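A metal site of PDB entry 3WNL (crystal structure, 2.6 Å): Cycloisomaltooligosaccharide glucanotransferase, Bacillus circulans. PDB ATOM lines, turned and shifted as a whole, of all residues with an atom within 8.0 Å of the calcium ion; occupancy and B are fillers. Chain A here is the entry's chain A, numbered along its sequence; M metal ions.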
ATOM      1  N   ARG A 386     -17.579   5.167  32.203  1.00  0.00           N
ATOM      2  CA  ARG A 386     -18.396   4.592  31.117  1.00  0.00           C
ATOM      3  C   ARG A 386     -17.967   5.009  29.702  1.00  0.00           C
ATOM      4  O   ARG A 386     -17.734   6.170  29.431  1.00  0.00           O
ATOM      5  CB  ARG A 386     -19.843   5.051  31.293  1.00  0.00           C
ATOM      6  CG  ARG A 386     -20.867   4.363  30.449  1.00  0.00           C
ATOM      7  CD  ARG A 386     -22.248   4.454  31.064  1.00  0.00           C
ATOM      8  NE  ARG A 386     -22.465   5.753  31.714  1.00  0.00           N
ATOM      9  CZ  ARG A 386     -23.604   6.122  32.302  1.00  0.00           C
ATOM     10  NH1 ARG A 386     -24.637   5.305  32.323  1.00  0.00           N
ATOM     11  NH2 ARG A 386     -23.703   7.322  32.854  1.00  0.00           N
ATOM     12  N   TYR A 387     -17.841   4.030  28.812  1.00  0.00           N
ATOM     13  CA  TYR A 387     -17.629   4.307  27.407  1.00  0.00           C
ATOM     14  C   TYR A 387     -18.808   3.746  26.621  1.00  0.00           C
ATOM     15  O   TYR A 387     -18.976   2.524  26.527  1.00  0.00           O
ATOM     16  CB  TYR A 387     -16.365   3.625  26.947  1.00  0.00           C
ATOM     17  CG  TYR A 387     -15.074   4.208  27.495  1.00  0.00           C
ATOM     18  CD1 TYR A 387     -14.557   3.788  28.728  1.00  0.00           C
ATOM     19  CD2 TYR A 387     -14.327   5.124  26.759  1.00  0.00           C
ATOM     20  CE1 TYR A 387     -13.358   4.291  29.224  1.00  0.00           C
ATOM     21  CE2 TYR A 387     -13.120   5.632  27.249  1.00  0.00           C
ATOM     22  CZ  TYR A 387     -12.639   5.225  28.486  1.00  0.00           C
ATOM     23  OH  TYR A 387     -11.433   5.726  28.970  1.00  0.00           O
ATOM     24  N   GLU A 388     -19.611   4.649  26.045  1.00  0.00           N
ATOM     25  CA  GLU A 388     -20.841   4.227  25.364  1.00  0.00           C
ATOM     26  C   GLU A 388     -20.513   3.410  24.123  1.00  0.00           C
ATOM     27  O   GLU A 388     -19.567   3.737  23.375  1.00  0.00           O
ATOM     28  CB  GLU A 388     -21.683   5.444  25.000  1.00  0.00           C
ATOM     29  CG  GLU A 388     -22.199   6.244  26.191  1.00  0.00           C
ATOM     30  CD  GLU A 388     -23.228   5.518  27.061  1.00  0.00           C
ATOM     31  OE1 GLU A 388     -23.688   4.402  26.697  1.00  0.00           O
ATOM     32  OE2 GLU A 388     -23.591   6.119  28.097  1.00  0.00           O
ATOM     33  N   ALA A 389     -21.253   2.339  23.901  1.00  0.00           N
ATOM     34  CA  ALA A 389     -20.917   1.441  22.817  1.00  0.00           C
ATOM     35  C   ALA A 389     -21.349   2.045  21.484  1.00  0.00           C
ATOM     36  O   ALA A 389     -20.688   1.851  20.454  1.00  0.00           O
ATOM     37  CB  ALA A 389     -21.516   0.092  23.019  1.00  0.00           C
ATOM     38  N   GLU A 390     -22.412   2.821  21.519  1.00  0.00           N
ATOM     39  CA  GLU A 390     -22.767   3.650  20.377  1.00  0.00           C
ATOM     40  C   GLU A 390     -21.694   4.693  19.984  1.00  0.00           C
ATOM     41  O   GLU A 390     -21.696   5.165  18.890  1.00  0.00           O
ATOM     42  CB  GLU A 390     -24.132   4.320  20.614  1.00  0.00           C
ATOM     43  CG  GLU A 390     -24.182   5.225  21.821  1.00  0.00           C
ATOM     44  CD  GLU A 390     -24.637   4.527  23.098  1.00  0.00           C
ATOM     45  OE1 GLU A 390     -24.390   3.298  23.275  1.00  0.00           O
ATOM     46  OE2 GLU A 390     -25.235   5.219  23.974  1.00  0.00           O
ATOM     47  N   SER A 391     -20.784   5.052  20.880  1.00  0.00           N
ATOM     48  CA  SER A 391     -19.724   6.036  20.550  1.00  0.00           C
ATOM     49  C   SER A 391     -18.374   5.399  20.178  1.00  0.00           C
ATOM     50  O   SER A 391     -17.369   6.108  19.997  1.00  0.00           O
ATOM     51  CB  SER A 391     -19.521   7.003  21.709  1.00  0.00           C
ATOM     52  OG  SER A 391     -20.744   7.631  21.960  1.00  0.00           O
ATOM     53  N   ASN A 400     -28.894   1.423  17.621  1.00  0.00           N
ATOM     54  CA  ASN A 400     -30.317   1.357  17.678  1.00  0.00           C
ATOM     55  C   ASN A 400     -30.798   1.954  18.977  1.00  0.00           C
ATOM     56  O   ASN A 400     -29.969   2.294  19.829  1.00  0.00           O
ATOM     57  CB  ASN A 400     -30.780  -0.085  17.541  1.00  0.00           C
ATOM     58  CG  ASN A 400     -32.092  -0.167  16.845  1.00  0.00           C
ATOM     59  OD1 ASN A 400     -32.976   0.622  17.111  1.00  0.00           O
ATOM     60  ND2 ASN A 400     -32.206  -1.065  15.925  1.00  0.00           N
ATOM     61  N   GLY A 405     -34.267   1.598  28.633  1.00  0.00           N
ATOM     62  CA  GLY A 405     -33.272   1.379  29.708  1.00  0.00           C
ATOM     63  C   GLY A 405     -31.782   1.380  29.304  1.00  0.00           C
ATOM     64  O   GLY A 405     -30.948   0.878  30.037  1.00  0.00           O
ATOM     65  N   TYR A 406     -31.440   1.912  28.127  1.00  0.00           N
ATOM     66  CA  TYR A 406     -30.021   2.022  27.762  1.00  0.00           C
ATOM     67  C   TYR A 406     -29.490   3.303  28.368  1.00  0.00           C
ATOM     68  O   TYR A 406     -30.248   4.191  28.675  1.00  0.00           O
ATOM     69  CB  TYR A 406     -29.799   2.027  26.234  1.00  0.00           C
ATOM     70  CG  TYR A 406     -30.587   3.074  25.491  1.00  0.00           C
ATOM     71  CD1 TYR A 406     -30.173   4.411  25.481  1.00  0.00           C
ATOM     72  CD2 TYR A 406     -31.751   2.737  24.801  1.00  0.00           C
ATOM     73  CE1 TYR A 406     -30.903   5.380  24.799  1.00  0.00           C
ATOM     74  CE2 TYR A 406     -32.475   3.694  24.117  1.00  0.00           C
ATOM     75  CZ  TYR A 406     -32.053   5.007  24.132  1.00  0.00           C
ATOM     76  OH  TYR A 406     -32.776   5.954  23.458  1.00  0.00           O
ATOM     77  N   THR A 407     -28.186   3.379  28.531  1.00  0.00           N
ATOM     78  CA  THR A 407     -27.540   4.632  28.862  1.00  0.00           C
ATOM     79  C   THR A 407     -27.082   5.325  27.532  1.00  0.00           C
ATOM     80  O   THR A 407     -26.984   4.687  26.462  1.00  0.00           O
ATOM     81  CB  THR A 407     -26.359   4.394  29.864  1.00  0.00           C
ATOM     82  OG1 THR A 407     -25.225   3.827  29.194  1.00  0.00           O
ATOM     83  CG2 THR A 407     -26.788   3.459  31.010  1.00  0.00           C
ATOM     84  N   GLY A 408     -26.848   6.635  27.600  1.00  0.00           N
ATOM     85  CA  GLY A 408     -26.454   7.409  26.438  1.00  0.00           C
ATOM     86  C   GLY A 408     -27.542   7.569  25.378  1.00  0.00           C
ATOM     87  O   GLY A 408     -28.698   7.767  25.697  1.00  0.00           O
ATOM     88  N   SER A 409     -27.149   7.470  24.117  1.00  0.00           N
ATOM     89  CA  SER A 409     -28.033   7.711  22.980  1.00  0.00           C
ATOM     90  C   SER A 409     -28.537   6.412  22.376  1.00  0.00           C
ATOM     91  O   SER A 409     -29.352   6.429  21.424  1.00  0.00           O
ATOM     92  CB  SER A 409     -27.299   8.529  21.897  1.00  0.00           C
ATOM     93  OG  SER A 409     -26.199   7.795  21.333  1.00  0.00           O
ATOM     94  N   GLY A 410     -28.071   5.283  22.905  1.00  0.00           N
ATOM     95  CA  GLY A 410     -28.652   4.004  22.507  1.00  0.00           C
ATOM     96  C   GLY A 410     -27.716   2.847  22.768  1.00  0.00           C
ATOM     97  O   GLY A 410     -27.066   2.758  23.814  1.00  0.00           O
ATOM     98  N   PHE A 411     -27.663   1.939  21.812  1.00  0.00           N
ATOM     99  CA  PHE A 411     -26.847   0.777  21.976  1.00  0.00           C
ATOM    100  C   PHE A 411     -26.585   0.096  20.642  1.00  0.00           C
ATOM    101  O   PHE A 411     -27.139   0.461  19.602  1.00  0.00           O
ATOM    102  CB  PHE A 411     -27.553  -0.188  22.918  1.00  0.00           C
ATOM    103  CG  PHE A 411     -28.916  -0.574  22.462  1.00  0.00           C
ATOM    104  CD1 PHE A 411     -30.009   0.171  22.810  1.00  0.00           C
ATOM    105  CD2 PHE A 411     -29.085  -1.696  21.681  1.00  0.00           C
ATOM    106  CE1 PHE A 411     -31.285  -0.207  22.379  1.00  0.00           C
ATOM    107  CE2 PHE A 411     -30.340  -2.086  21.246  1.00  0.00           C
ATOM    108  CZ  PHE A 411     -31.440  -1.329  21.597  1.00  0.00           C
ATOM    109  N   VAL A 412     -25.729  -0.919  20.690  1.00  0.00           N
ATOM    110  CA  VAL A 412     -25.402  -1.649  19.503  1.00  0.00           C
ATOM    111  C   VAL A 412     -26.195  -2.950  19.543  1.00  0.00           C
ATOM    112  O   VAL A 412     -26.125  -3.681  20.524  1.00  0.00           O
ATOM    113  CB  VAL A 412     -23.870  -1.876  19.409  1.00  0.00           C
ATOM    114  CG1 VAL A 412     -23.533  -2.820  18.272  1.00  0.00           C
ATOM    115  CG2 VAL A 412     -23.140  -0.531  19.257  1.00  0.00           C
ATOM    116  N   ARG A 439     -22.273  -3.792  29.790  1.00  0.00           N
ATOM    117  CA  ARG A 439     -23.687  -3.810  29.970  1.00  0.00           C
ATOM    118  C   ARG A 439     -24.322  -4.249  28.665  1.00  0.00           C
ATOM    119  O   ARG A 439     -23.979  -3.740  27.613  1.00  0.00           O
ATOM    120  CB  ARG A 439     -24.201  -2.430  30.376  1.00  0.00           C
ATOM    121  CG  ARG A 439     -25.668  -2.442  30.817  1.00  0.00           C
ATOM    122  CD  ARG A 439     -25.928  -1.289  31.740  1.00  0.00           C
ATOM    123  NE  ARG A 439     -27.241  -1.316  32.357  1.00  0.00           N
ATOM    124  CZ  ARG A 439     -28.335  -0.671  31.907  1.00  0.00           C
ATOM    125  NH1 ARG A 439     -28.338   0.052  30.768  1.00  0.00           N
ATOM    126  NH2 ARG A 439     -29.462  -0.766  32.590  1.00  0.00           N
ATOM    127  N   TRP A 473     -31.495  -5.130  31.033  1.00  0.00           N
ATOM    128  CA  TRP A 473     -30.031  -4.976  31.010  1.00  0.00           C
ATOM    129  C   TRP A 473     -29.350  -5.549  32.227  1.00  0.00           C
ATOM    130  O   TRP A 473     -29.754  -5.294  33.355  1.00  0.00           O
ATOM    131  CB  TRP A 473     -29.650  -3.510  30.869  1.00  0.00           C
ATOM    132  CG  TRP A 473     -30.340  -2.903  29.704  1.00  0.00           C
ATOM    133  CD1 TRP A 473     -31.513  -2.215  29.727  1.00  0.00           C
ATOM    134  CD2 TRP A 473     -29.969  -3.007  28.320  1.00  0.00           C
ATOM    135  NE1 TRP A 473     -31.872  -1.849  28.447  1.00  0.00           N
ATOM    136  CE2 TRP A 473     -30.948  -2.336  27.569  1.00  0.00           C
ATOM    137  CE3 TRP A 473     -28.878  -3.574  27.654  1.00  0.00           C
ATOM    138  CZ2 TRP A 473     -30.867  -2.205  26.186  1.00  0.00           C
ATOM    139  CZ3 TRP A 473     -28.812  -3.476  26.278  1.00  0.00           C
ATOM    140  CH2 TRP A 473     -29.809  -2.787  25.554  1.00  0.00           C
ATOM    141  N   LEU A 504     -25.275  -4.464  22.992  1.00  0.00           N
ATOM    142  CA  LEU A 504     -24.227  -3.981  23.874  1.00  0.00           C
ATOM    143  C   LEU A 504     -24.498  -2.560  24.183  1.00  0.00           C
ATOM    144  O   LEU A 504     -24.667  -1.748  23.273  1.00  0.00           O
ATOM    145  CB  LEU A 504     -22.889  -4.085  23.161  1.00  0.00           C
ATOM    146  CG  LEU A 504     -21.608  -3.806  23.928  1.00  0.00           C
ATOM    147  CD1 LEU A 504     -21.460  -4.691  25.180  1.00  0.00           C
ATOM    148  CD2 LEU A 504     -20.418  -4.025  22.973  1.00  0.00           C
ATOM    149  N   ASP A 505     -24.563  -2.235  25.463  1.00  0.00           N
ATOM    150  CA  ASP A 505     -24.912  -0.870  25.809  1.00  0.00           C
ATOM    151  C   ASP A 505     -23.657  -0.016  26.003  1.00  0.00           C
ATOM    152  O   ASP A 505     -23.612   1.139  25.568  1.00  0.00           O
ATOM    153  CB  ASP A 505     -25.805  -0.813  27.049  1.00  0.00           C
ATOM    154  CG  ASP A 505     -26.426   0.557  27.244  1.00  0.00           C
ATOM    155  OD1 ASP A 505     -26.777   1.201  26.238  1.00  0.00           O
ATOM    156  OD2 ASP A 505     -26.553   1.014  28.377  1.00  0.00           O
ATOM    157  N   SER A 506     -22.646  -0.589  26.661  1.00  0.00           N
ATOM    158  CA  SER A 506     -21.515   0.196  27.057  1.00  0.00           C
ATOM    159  C   SER A 506     -20.422  -0.670  27.609  1.00  0.00           C
ATOM    160  O   SER A 506     -20.676  -1.818  27.882  1.00  0.00           O
ATOM    161  CB  SER A 506     -21.926   1.167  28.144  1.00  0.00           C
ATOM    162  OG  SER A 506     -22.417   0.421  29.228  1.00  0.00           O
ATOM    163  N   LEU A 507     -19.210  -0.093  27.734  1.00  0.00           N
ATOM    164  CA  LEU A 507     -18.120  -0.652  28.501  1.00  0.00           C
ATOM    165  C   LEU A 507     -17.819   0.260  29.664  1.00  0.00           C
ATOM    166  O   LEU A 507     -17.845   1.473  29.511  1.00  0.00           O
ATOM    167  CB  LEU A 507     -16.867  -0.721  27.658  1.00  0.00           C
ATOM    168  CG  LEU A 507     -15.526  -0.915  28.393  1.00  0.00           C
ATOM    169  CD1 LEU A 507     -15.401  -2.305  29.057  1.00  0.00           C
ATOM    170  CD2 LEU A 507     -14.424  -0.668  27.378  1.00  0.00           C
HETATM  171 CA    CA M   1     -25.441   3.109  25.547  1.00  0.00          CA
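OE2 of Glu 388 is in salt-bridge range of NE of Arg 386, at 3.8 Å.
OE2 of Glu 390 sits close to N of Ser 409, 3.0 Å away.
The backbone carbonyl oxygen (O) of Asp 505 lies close to the backbone NH (N) of Ala 389.
The guanidinium group of Arg 439 lies within salt-bridge range of the side-chain carboxylate of Asp 505, 3.1 Å away.
The side-chain carboxylate (OE2) of Glu 388 sits at hydrogen-bond distance from the backbone NH (N) of Gly 408 (3.3 Å).
O of Thr 407 is bound to the calcium ion (2.4 Å).
The calcium ion is bound by the backbone carbonyl oxygen (O) of Gly 410.
The calcium ion is bound by OD1 of Asp 505 (2.4 Å).
The calcium ion is bound by OE1 of Glu 388 (2.5 Å).
The calcium ion is bound by OE1 of Glu 390.
OE2 of Glu 390 is bound to the calcium ion (2.6 Å).
The calcium ion is bound by O of Asp 505.
The calcium ion has seven donor atoms within binding distance.
Within 4 Å of the calcium ion: Glu 388, Glu 390, Thr 407, Gly 410 and Asp 505.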
